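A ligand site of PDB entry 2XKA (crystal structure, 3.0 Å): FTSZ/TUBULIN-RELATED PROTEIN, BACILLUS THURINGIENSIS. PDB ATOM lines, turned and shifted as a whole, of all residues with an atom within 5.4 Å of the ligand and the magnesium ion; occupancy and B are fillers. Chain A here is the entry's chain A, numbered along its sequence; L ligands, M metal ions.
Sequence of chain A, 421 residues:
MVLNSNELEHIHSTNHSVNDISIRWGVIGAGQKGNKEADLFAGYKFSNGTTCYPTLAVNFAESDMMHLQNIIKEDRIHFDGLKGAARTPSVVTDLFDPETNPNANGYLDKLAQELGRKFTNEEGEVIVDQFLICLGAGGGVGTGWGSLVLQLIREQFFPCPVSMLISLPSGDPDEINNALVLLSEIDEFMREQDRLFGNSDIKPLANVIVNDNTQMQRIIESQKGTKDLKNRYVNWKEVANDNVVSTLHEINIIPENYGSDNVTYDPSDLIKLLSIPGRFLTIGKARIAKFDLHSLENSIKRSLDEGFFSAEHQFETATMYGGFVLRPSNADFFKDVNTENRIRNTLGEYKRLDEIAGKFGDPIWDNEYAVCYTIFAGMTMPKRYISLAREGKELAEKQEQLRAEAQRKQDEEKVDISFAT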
ATOM      1  N   ALA A  30      12.053  -4.741 -23.285  1.00  0.00           N
ATOM      2  CA  ALA A  30      11.730  -6.165 -23.164  1.00  0.00           C
ATOM      3  C   ALA A  30      11.564  -6.535 -21.701  1.00  0.00           C
ATOM      4  O   ALA A  30      12.301  -6.063 -20.835  1.00  0.00           O
ATOM      5  CB  ALA A  30      12.811  -6.995 -23.775  1.00  0.00           C
ATOM      6  N   GLY A  31      10.613  -7.406 -21.417  1.00  0.00           N
ATOM      7  CA  GLY A  31      10.326  -7.790 -20.036  1.00  0.00           C
ATOM      8  C   GLY A  31       9.573  -6.664 -19.379  1.00  0.00           C
ATOM      9  O   GLY A  31       9.365  -5.627 -19.984  1.00  0.00           O
ATOM     10  N   GLN A  32       9.208  -6.873 -18.116  1.00  0.00           N
ATOM     11  CA  GLN A  32       8.306  -5.966 -17.401  1.00  0.00           C
ATOM     12  C   GLN A  32       8.984  -4.646 -17.102  1.00  0.00           C
ATOM     13  O   GLN A  32       8.431  -3.589 -17.377  1.00  0.00           O
ATOM     14  CB  GLN A  32       7.812  -6.618 -16.095  1.00  0.00           C
ATOM     15  CG  GLN A  32       6.313  -6.499 -15.871  1.00  0.00           C
ATOM     16  CD  GLN A  32       5.531  -7.764 -16.188  1.00  0.00           C
ATOM     17  OE1 GLN A  32       5.972  -8.906 -15.939  1.00  0.00           O
ATOM     18  NE2 GLN A  32       4.328  -7.569 -16.702  1.00  0.00           N
ATOM     19  N   LYS A  33      10.181  -4.723 -16.539  1.00  0.00           N
ATOM     20  CA  LYS A  33      11.008  -3.543 -16.253  1.00  0.00           C
ATOM     21  C   LYS A  33      11.244  -2.730 -17.525  1.00  0.00           C
ATOM     22  O   LYS A  33      10.969  -1.537 -17.576  1.00  0.00           O
ATOM     23  CB  LYS A  33      12.366  -3.936 -15.679  1.00  0.00           C
ATOM     24  CG  LYS A  33      13.236  -2.740 -15.234  1.00  0.00           C
ATOM     25  CD  LYS A  33      14.210  -2.225 -16.319  1.00  0.00           C
ATOM     26  CE  LYS A  33      15.308  -1.351 -15.698  1.00  0.00           C
ATOM     27  NZ  LYS A  33      16.470  -1.011 -16.623  1.00  0.00           N
ATOM     28  N   GLY A  34      11.744  -3.399 -18.554  1.00  0.00           N
ATOM     29  CA  GLY A  34      11.968  -2.773 -19.838  1.00  0.00           C
ATOM     30  C   GLY A  34      10.728  -2.108 -20.388  1.00  0.00           C
ATOM     31  O   GLY A  34      10.823  -1.009 -20.923  1.00  0.00           O
ATOM     32  N   LYS A  36       8.247  -0.837 -18.721  1.00  0.00           N
ATOM     33  CA  LYS A  36       7.907   0.339 -17.944  1.00  0.00           C
ATOM     34  C   LYS A  36       8.807   1.511 -18.275  1.00  0.00           C
ATOM     35  O   LYS A  36       8.314   2.638 -18.380  1.00  0.00           O
ATOM     36  CB  LYS A  36       7.955   0.022 -16.455  1.00  0.00           C
ATOM     37  CG  LYS A  36       6.820  -0.881 -16.032  1.00  0.00           C
ATOM     38  CD  LYS A  36       6.661  -0.948 -14.534  1.00  0.00           C
ATOM     39  CE  LYS A  36       7.579  -1.984 -13.909  1.00  0.00           C
ATOM     40  NZ  LYS A  36       7.636  -1.803 -12.432  1.00  0.00           N
ATOM     41  N   ASN A  59       7.120  -8.441 -24.861  1.00  0.00           N
ATOM     42  CA  ASN A  59       6.996  -9.361 -23.744  1.00  0.00           C
ATOM     43  C   ASN A  59       6.494 -10.774 -24.112  1.00  0.00           C
ATOM     44  O   ASN A  59       6.260 -11.078 -25.266  1.00  0.00           O
ATOM     45  CB  ASN A  59       6.126  -8.754 -22.642  1.00  0.00           C
ATOM     46  CG  ASN A  59       6.677  -9.035 -21.264  1.00  0.00           C
ATOM     47  OD1 ASN A  59       7.120 -10.152 -20.970  1.00  0.00           O
ATOM     48  ND2 ASN A  59       6.673  -8.020 -20.407  1.00  0.00           N
ATOM     49  N   ASP A  64       1.084  -9.551 -19.844  1.00  0.00           N
ATOM     50  CA  ASP A  64       2.169  -8.743 -19.251  1.00  0.00           C
ATOM     51  C   ASP A  64       2.020  -7.236 -19.537  1.00  0.00           C
ATOM     52  O   ASP A  64       2.331  -6.422 -18.674  1.00  0.00           O
ATOM     53  CB  ASP A  64       3.566  -9.251 -19.686  1.00  0.00           C
ATOM     54  CG  ASP A  64       4.173 -10.296 -18.690  1.00  0.00           C
ATOM     55  OD1 ASP A  64       3.441 -11.206 -18.233  1.00  0.00           O
ATOM     56  OD2 ASP A  64       5.388 -10.213 -18.361  1.00  0.00           O
ATOM     57  N   ARG A  87       9.513 -20.104 -17.482  1.00  0.00           N
ATOM     58  CA  ARG A  87       9.899 -18.750 -17.895  1.00  0.00           C
ATOM     59  C   ARG A  87      11.346 -18.460 -17.490  1.00  0.00           C
ATOM     60  O   ARG A  87      11.596 -17.976 -16.382  1.00  0.00           O
ATOM     61  CB  ARG A  87       8.967 -17.714 -17.231  1.00  0.00           C
ATOM     62  CG  ARG A  87       7.503 -17.798 -17.644  1.00  0.00           C
ATOM     63  CD  ARG A  87       6.818 -16.423 -17.535  1.00  0.00           C
ATOM     64  NE  ARG A  87       5.416 -16.468 -17.982  1.00  0.00           N
ATOM     65  CZ  ARG A  87       4.557 -15.450 -17.902  1.00  0.00           C
ATOM     66  NH1 ARG A  87       3.315 -15.621 -18.345  1.00  0.00           N
ATOM     67  NH2 ARG A  87       4.926 -14.280 -17.379  1.00  0.00           N
ATOM     68  N   GLY A 136      15.525  -5.550 -17.573  1.00  0.00           N
ATOM     69  CA  GLY A 136      15.767  -5.815 -16.174  1.00  0.00           C
ATOM     70  C   GLY A 136      16.428  -7.182 -16.052  1.00  0.00           C
ATOM     71  O   GLY A 136      15.765  -8.211 -16.216  1.00  0.00           O
ATOM     72  N   ALA A 137      17.738  -7.206 -15.830  1.00  0.00           N
ATOM     73  CA  ALA A 137      18.469  -8.475 -15.710  1.00  0.00           C
ATOM     74  C   ALA A 137      17.947  -9.221 -14.502  1.00  0.00           C
ATOM     75  O   ALA A 137      17.756  -8.646 -13.410  1.00  0.00           O
ATOM     76  CB  ALA A 137      19.961  -8.244 -15.558  1.00  0.00           C
ATOM     77  N   GLY A 138      17.722 -10.529 -14.698  1.00  0.00           N
ATOM     78  CA  GLY A 138      17.214 -11.407 -13.627  1.00  0.00           C
ATOM     79  C   GLY A 138      16.019 -12.239 -14.039  1.00  0.00           C
ATOM     80  O   GLY A 138      15.955 -13.432 -13.731  1.00  0.00           O
ATOM     81  N   GLY A 139      15.083 -11.607 -14.725  1.00  0.00           N
ATOM     82  CA  GLY A 139      13.869 -12.286 -15.156  1.00  0.00           C
ATOM     83  C   GLY A 139      14.136 -13.200 -16.321  1.00  0.00           C
ATOM     84  O   GLY A 139      15.279 -13.283 -16.786  1.00  0.00           O
ATOM     85  N   GLY A 140      13.103 -13.888 -16.783  1.00  0.00           N
ATOM     86  CA  GLY A 140      13.216 -14.728 -17.974  1.00  0.00           C
ATOM     87  C   GLY A 140      13.209 -13.900 -19.241  1.00  0.00           C
ATOM     88  O   GLY A 140      14.208 -13.837 -19.963  1.00  0.00           O
ATOM     89  N   VAL A 141      12.076 -13.248 -19.488  1.00  0.00           N
ATOM     90  CA  VAL A 141      11.846 -12.501 -20.735  1.00  0.00           C
ATOM     91  C   VAL A 141      12.900 -11.441 -20.998  1.00  0.00           C
ATOM     92  O   VAL A 141      13.463 -11.377 -22.084  1.00  0.00           O
ATOM     93  CB  VAL A 141      10.460 -11.837 -20.735  1.00  0.00           C
ATOM     94  CG1 VAL A 141      10.289 -10.967 -21.942  1.00  0.00           C
ATOM     95  CG2 VAL A 141       9.380 -12.886 -20.713  1.00  0.00           C
ATOM     96  N   GLY A 142      13.172 -10.624 -19.990  1.00  0.00           N
ATOM     97  CA  GLY A 142      14.164  -9.551 -20.106  1.00  0.00           C
ATOM     98  C   GLY A 142      15.584 -10.044 -20.372  1.00  0.00           C
ATOM     99  O   GLY A 142      16.220  -9.674 -21.353  1.00  0.00           O
ATOM    100  N   THR A 143      16.067 -10.884 -19.474  1.00  0.00           N
ATOM    101  CA  THR A 143      17.429 -11.416 -19.592  1.00  0.00           C
ATOM    102  C   THR A 143      17.620 -12.167 -20.890  1.00  0.00           C
ATOM    103  O   THR A 143      18.683 -12.107 -21.501  1.00  0.00           O
ATOM    104  CB  THR A 143      17.786 -12.342 -18.430  1.00  0.00           C
ATOM    105  OG1 THR A 143      17.410 -11.712 -17.190  1.00  0.00           O
ATOM    106  CG2 THR A 143      19.270 -12.645 -18.428  1.00  0.00           C
ATOM    107  N   SER A 167      19.445  -3.169 -15.899  1.00  0.00           N
ATOM    108  CA  SER A 167      19.294  -3.012 -14.470  1.00  0.00           C
ATOM    109  C   SER A 167      19.703  -4.307 -13.791  1.00  0.00           C
ATOM    110  O   SER A 167      19.283  -5.390 -14.210  1.00  0.00           O
ATOM    111  CB  SER A 167      17.828  -2.672 -14.169  1.00  0.00           C
ATOM    112  OG  SER A 167      17.309  -3.310 -13.018  1.00  0.00           O
ATOM    113  N   LEU A 168      20.516  -4.209 -12.743  1.00  0.00           N
ATOM    114  CA  LEU A 168      21.004  -5.386 -12.018  1.00  0.00           C
ATOM    115  C   LEU A 168      20.090  -5.754 -10.848  1.00  0.00           C
ATOM    116  O   LEU A 168      19.618  -4.887 -10.131  1.00  0.00           O
ATOM    117  CB  LEU A 168      22.436  -5.151 -11.522  1.00  0.00           C
ATOM    118  CG  LEU A 168      23.475  -4.898 -12.625  1.00  0.00           C
ATOM    119  CD1 LEU A 168      24.858  -4.789 -12.001  1.00  0.00           C
ATOM    120  CD2 LEU A 168      23.458  -5.998 -13.685  1.00  0.00           C
ATOM    121  N   PRO A 169      19.852  -7.064 -10.651  1.00  0.00           N
ATOM    122  CA  PRO A 169      18.824  -7.544  -9.740  1.00  0.00           C
ATOM    123  C   PRO A 169      19.181  -7.368  -8.282  1.00  0.00           C
ATOM    124  O   PRO A 169      20.368  -7.326  -7.912  1.00  0.00           O
ATOM    125  CB  PRO A 169      18.730  -9.021 -10.080  1.00  0.00           C
ATOM    126  CG  PRO A 169      20.099  -9.374 -10.498  1.00  0.00           C
ATOM    127  CD  PRO A 169      20.653  -8.175 -11.199  1.00  0.00           C
ATOM    128  N   SER A 170      18.141  -7.290  -7.457  1.00  0.00           N
ATOM    129  CA  SER A 170      18.297  -6.964  -6.039  1.00  0.00           C
ATOM    130  C   SER A 170      18.896  -8.099  -5.230  1.00  0.00           C
ATOM    131  O   SER A 170      19.992  -7.948  -4.715  1.00  0.00           O
ATOM    132  CB  SER A 170      16.971  -6.524  -5.429  1.00  0.00           C
ATOM    133  OG  SER A 170      17.206  -5.880  -4.193  1.00  0.00           O
ATOM    134  N   GLU A 175      17.806 -15.110  -9.995  1.00  0.00           N
ATOM    135  CA  GLU A 175      17.956 -13.840 -10.704  1.00  0.00           C
ATOM    136  C   GLU A 175      19.424 -13.413 -10.831  1.00  0.00           C
ATOM    137  O   GLU A 175      19.847 -12.971 -11.897  1.00  0.00           O
ATOM    138  CB  GLU A 175      17.158 -12.711 -10.017  1.00  0.00           C
ATOM    139  CG  GLU A 175      15.657 -12.734 -10.292  1.00  0.00           C
ATOM    140  CD  GLU A 175      14.901 -11.601  -9.602  1.00  0.00           C
ATOM    141  OE1 GLU A 175      13.646 -11.612  -9.650  1.00  0.00           O
ATOM    142  OE2 GLU A 175      15.544 -10.696  -9.017  1.00  0.00           O
ATOM    143  N   ASN A 213      19.949  -2.278  -8.675  1.00  0.00           N
ATOM    144  CA  ASN A 213      18.736  -2.158  -7.881  1.00  0.00           C
ATOM    145  C   ASN A 213      18.994  -2.000  -6.397  1.00  0.00           C
ATOM    146  O   ASN A 213      18.209  -1.380  -5.699  1.00  0.00           O
ATOM    147  CB  ASN A 213      17.785  -3.335  -8.123  1.00  0.00           C
ATOM    148  CG  ASN A 213      16.951  -3.165  -9.379  1.00  0.00           C
ATOM    149  OD1 ASN A 213      16.859  -2.094  -9.957  1.00  0.00           O
ATOM    150  ND2 ASN A 213      16.325  -4.247  -9.801  1.00  0.00           N
ATOM    151  N   MET A 216      20.088   1.624  -5.853  1.00  0.00           N
ATOM    152  CA  MET A 216      19.002   2.538  -6.167  1.00  0.00           C
ATOM    153  C   MET A 216      17.998   2.602  -5.036  1.00  0.00           C
ATOM    154  O   MET A 216      17.466   3.678  -4.741  1.00  0.00           O
ATOM    155  CB  MET A 216      18.318   2.150  -7.483  1.00  0.00           C
ATOM    156  CG  MET A 216      19.127   2.552  -8.731  1.00  0.00           C
ATOM    157  SD  MET A 216      18.214   2.477 -10.292  1.00  0.00           S
ATOM    158  CE  MET A 216      18.033   0.705 -10.456  1.00  0.00           C
ATOM    159  N   TRP A 236       9.368   2.261  -4.922  1.00  0.00           N
ATOM    160  CA  TRP A 236      10.744   2.612  -5.282  1.00  0.00           C
ATOM    161  C   TRP A 236      11.116   2.408  -6.759  1.00  0.00           C
ATOM    162  O   TRP A 236      11.916   3.169  -7.308  1.00  0.00           O
ATOM    163  CB  TRP A 236      11.756   1.903  -4.375  1.00  0.00           C
ATOM    164  CG  TRP A 236      11.924   0.468  -4.647  1.00  0.00           C
ATOM    165  CD1 TRP A 236      11.297  -0.566  -4.019  1.00  0.00           C
ATOM    166  CD2 TRP A 236      12.785  -0.135  -5.627  1.00  0.00           C
ATOM    167  NE1 TRP A 236      11.713  -1.765  -4.539  1.00  0.00           N
ATOM    168  CE2 TRP A 236      12.624  -1.524  -5.524  1.00  0.00           C
ATOM    169  CE3 TRP A 236      13.670   0.384  -6.575  1.00  0.00           C
ATOM    170  CZ2 TRP A 236      13.327  -2.417  -6.342  1.00  0.00           C
ATOM    171  CZ3 TRP A 236      14.372  -0.502  -7.384  1.00  0.00           C
ATOM    172  CH2 TRP A 236      14.195  -1.891  -7.258  1.00  0.00           C
ATOM    173  N   LYS A 237      10.543   1.378  -7.392  1.00  0.00           N
ATOM    174  CA  LYS A 237      10.776   1.100  -8.819  1.00  0.00           C
ATOM    175  C   LYS A 237      10.311   2.237  -9.725  1.00  0.00           C
ATOM    176  O   LYS A 237      10.999   2.631 -10.655  1.00  0.00           O
ATOM    177  CB  LYS A 237      10.044  -0.176  -9.222  1.00  0.00           C
ATOM    178  CG  LYS A 237      10.672  -1.446  -8.659  1.00  0.00           C
ATOM    179  CD  LYS A 237       9.844  -2.663  -8.981  1.00  0.00           C
ATOM    180  CE  LYS A 237      10.401  -3.882  -8.277  1.00  0.00           C
ATOM    181  NZ  LYS A 237       9.547  -5.076  -8.557  1.00  0.00           N
ATOM    182  N   GLU A 238       9.130   2.734  -9.417  1.00  0.00           N
ATOM    183  CA  GLU A 238       8.529   3.868 -10.100  1.00  0.00           C
ATOM    184  C   GLU A 238       9.406   5.125 -10.018  1.00  0.00           C
ATOM    185  O   GLU A 238       9.532   5.896 -10.982  1.00  0.00           O
ATOM    186  CB  GLU A 238       7.134   4.133  -9.505  1.00  0.00           C
ATOM    187  CG  GLU A 238       6.285   5.135 -10.247  1.00  0.00           C
ATOM    188  CD  GLU A 238       4.778   5.004  -9.920  1.00  0.00           C
ATOM    189  OE1 GLU A 238       4.354   3.936  -9.402  1.00  0.00           O
ATOM    190  OE2 GLU A 238       4.034   5.975 -10.207  1.00  0.00           O
ATOM    191  N   ALA A 240      12.853   5.071  -9.116  1.00  0.00           N
ATOM    192  CA  ALA A 240      14.110   4.740  -9.781  1.00  0.00           C
ATOM    193  C   ALA A 240      14.000   4.964 -11.296  1.00  0.00           C
ATOM    194  O   ALA A 240      14.851   5.599 -11.906  1.00  0.00           O
ATOM    195  CB  ALA A 240      14.510   3.294  -9.495  1.00  0.00           C
ATOM    196  N   ASN A 241      12.932   4.453 -11.874  1.00  0.00           N
ATOM    197  CA  ASN A 241      12.709   4.618 -13.322  1.00  0.00           C
ATOM    198  C   ASN A 241      12.638   6.079 -13.752  1.00  0.00           C
ATOM    199  O   ASN A 241      13.306   6.482 -14.703  1.00  0.00           O
ATOM    200  CB  ASN A 241      11.441   3.901 -13.755  1.00  0.00           C
ATOM    201  CG  ASN A 241      11.568   2.396 -13.664  1.00  0.00           C
ATOM    202  OD1 ASN A 241      12.670   1.859 -13.522  1.00  0.00           O
ATOM    203  ND2 ASN A 241      10.438   1.703 -13.757  1.00  0.00           N
HETATM  204  P1  LIG L   1       9.639 -12.905 -16.359  1.00  0.00           P
HETATM  205  O1  LIG L   1      10.800 -11.793 -16.292  1.00  0.00           O
HETATM  206  S1  LIG L   1       9.971 -13.872 -17.677  1.00  0.00           S
HETATM  207  O2  LIG L   1       9.772 -13.823 -15.145  1.00  0.00           O
HETATM  208  O3  LIG L   1       8.220 -12.328 -16.588  1.00  0.00           O
HETATM  209  P2  LIG L   1      10.638 -10.228 -16.662  1.00  0.00           P
HETATM  210  O4  LIG L   1       9.221  -9.773 -16.772  1.00  0.00           O
HETATM  211  O5  LIG L   1      11.406 -10.014 -17.899  1.00  0.00           O
HETATM  212  P3  LIG L   1      10.972  -8.243 -14.614  1.00  0.00           P
HETATM  213  O6  LIG L   1       9.600  -8.395 -14.052  1.00  0.00           O
HETATM  214  O7  LIG L   1      10.928  -7.054 -15.491  1.00  0.00           O
HETATM  215  O8  LIG L   1      11.447  -9.549 -15.438  1.00  0.00           O
HETATM  216  O9  LIG L   1      12.066  -8.112 -13.452  1.00  0.00           O
HETATM  217  C1  LIG L   1      13.386  -8.570 -13.657  1.00  0.00           C
HETATM  218  C2  LIG L   1      14.362  -7.855 -12.729  1.00  0.00           C
HETATM  219  O10 LIG L   1      14.185  -6.458 -12.795  1.00  0.00           O
HETATM  220  C3  LIG L   1      14.145  -8.207 -11.274  1.00  0.00           C
HETATM  221  O11 LIG L   1      15.362  -8.121 -10.592  1.00  0.00           O
HETATM  222  C4  LIG L   1      13.209  -7.132 -10.792  1.00  0.00           C
HETATM  223  O12 LIG L   1      13.377  -6.802  -9.452  1.00  0.00           O
HETATM  224  C5  LIG L   1      13.618  -5.951 -11.627  1.00  0.00           C
HETATM  225  N1  LIG L   1      12.490  -5.064 -11.926  1.00  0.00           N
HETATM  226  C6  LIG L   1      11.170  -5.329 -12.245  1.00  0.00           C
HETATM  227  N2  LIG L   1      10.520  -4.137 -12.421  1.00  0.00           N
HETATM  228  C7  LIG L   1      11.416  -3.128 -12.210  1.00  0.00           C
HETATM  229  C8  LIG L   1      11.365  -1.730 -12.235  1.00  0.00           C
HETATM  230  O13 LIG L   1      10.326  -1.153 -12.513  1.00  0.00           O
HETATM  231  N3  LIG L   1      12.478  -0.968 -11.982  1.00  0.00           N
HETATM  232  C9  LIG L   1      13.668  -1.595 -11.670  1.00  0.00           C
HETATM  233  N4  LIG L   1      14.788  -0.931 -11.406  1.00  0.00           N
HETATM  234  N5  LIG L   1      13.737  -2.956 -11.634  1.00  0.00           N
HETATM  235  C10 LIG L   1      12.638  -3.711 -11.902  1.00  0.00           C
HETATM  236 MG    MG M   1       7.423 -10.417 -15.650  1.00  0.00          MG
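The backbone NH of Lys 33 lies within hydrogen-bond range of an oxygen (O7) of the ligand, 2.7 Å away. N of Gly 142 sits at hydrogen-bond distance from O5 of the ligand, at 2.8 Å. The side-chain amide oxygen (OD1) of Asn 213 sits at hydrogen-bond distance from a nitrogen (N4) of the ligand (2.8 Å). O1 of the ligand is in hydrogen-bond range of N of Gly 140 (3.2 Å). O13 of the ligand sits at hydrogen-bond distance from NZ of Lys 36, 2.8 Å away. An oxygen (O13) of the ligand lies within hydrogen-bond range of the side-chain amide nitrogen (ND2) of Asn 241 (3.1 Å). O7 of the ligand is in hydrogen-bond range of N of Gln 32 (3.1 Å). S1 of the ligand sits close to N of Val 141, 2.8 Å away. An oxygen (O11) of the ligand lies within hydrogen-bond range of the side-chain carboxylate of Glu 175.
ND2 of Asn 241 lies close to O of Lys 237. The backbone carbonyl oxygen of Ser 167 lies within hydrogen-bond range of the backbone NH of Ala 137. The side-chain hydroxyl of Thr 143 sits at hydrogen-bond distance from the backbone carbonyl oxygen of Gly 139, 2.7 Å away. The side-chain hydroxyl of Ser 167 is in hydrogen-bond range of the side-chain amide oxygen of Asn 213. The side-chain carboxylate (OD1) of Asp 64 lies within salt-bridge range of the guanidinium group (NH2) of Arg 87 (3.5 Å). The side-chain amide oxygen (OD1) of Asn 59 lies close to the side-chain carboxylate (OD2) of Asp 64 (3.1 Å). The side-chain amide nitrogen of Gln 32 sits at hydrogen-bond distance from the backbone carbonyl oxygen of Asp 64 (3.0 Å). The backbone carbonyl oxygen (O) of Leu 168 is in hydrogen-bond range of the backbone NH (N) of Asn 213 (3.0 Å).
CA of Gly 31 touches O5 of the ligand, 3.3 Å away. OD2 of Asp 64 touches O3 of the ligand, 3.95 Å away. Arg 87 touches the ligand (NH2 to O3, 3.9 Å). Gly 136 touches the ligand (O to C1, 3.5 Å). Ala 137 touches the ligand (O to C2, 3.6 Å). Gly 139 touches the ligand. Ser 167 touches the ligand. CB of Pro 169 touches O11 of the ligand, 3.5 Å away. CE of Met 216 touches N4 of the ligand, 3.8 Å away. CB of Lys 237 touches O13 of the ligand (3.4 Å). Within 4 Å of the ligand: Gly 31, Gln 32, Lys 33, Lys 36, Asp 64, Arg 87, Gly 136, Ala 137, Gly 139, Gly 140, Val 141, Gly 142, Ser 167, Pro 169, Glu 175, Asn 213, Met 216, Lys 237 and Asn 241.
Merely in contact with the magnesium ion: Asp 64 (3.4 Å). The nearest printed residue that does not touch the magnesium ion is Arg 87 (4.9 Å).
The magnesium ion is bound by the side-chain amide oxygen of Gln 32 (2.1 Å), an oxygen (O4) of the ligand (2.2 Å) and an oxygen (O3) of the ligand (2.3 Å).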
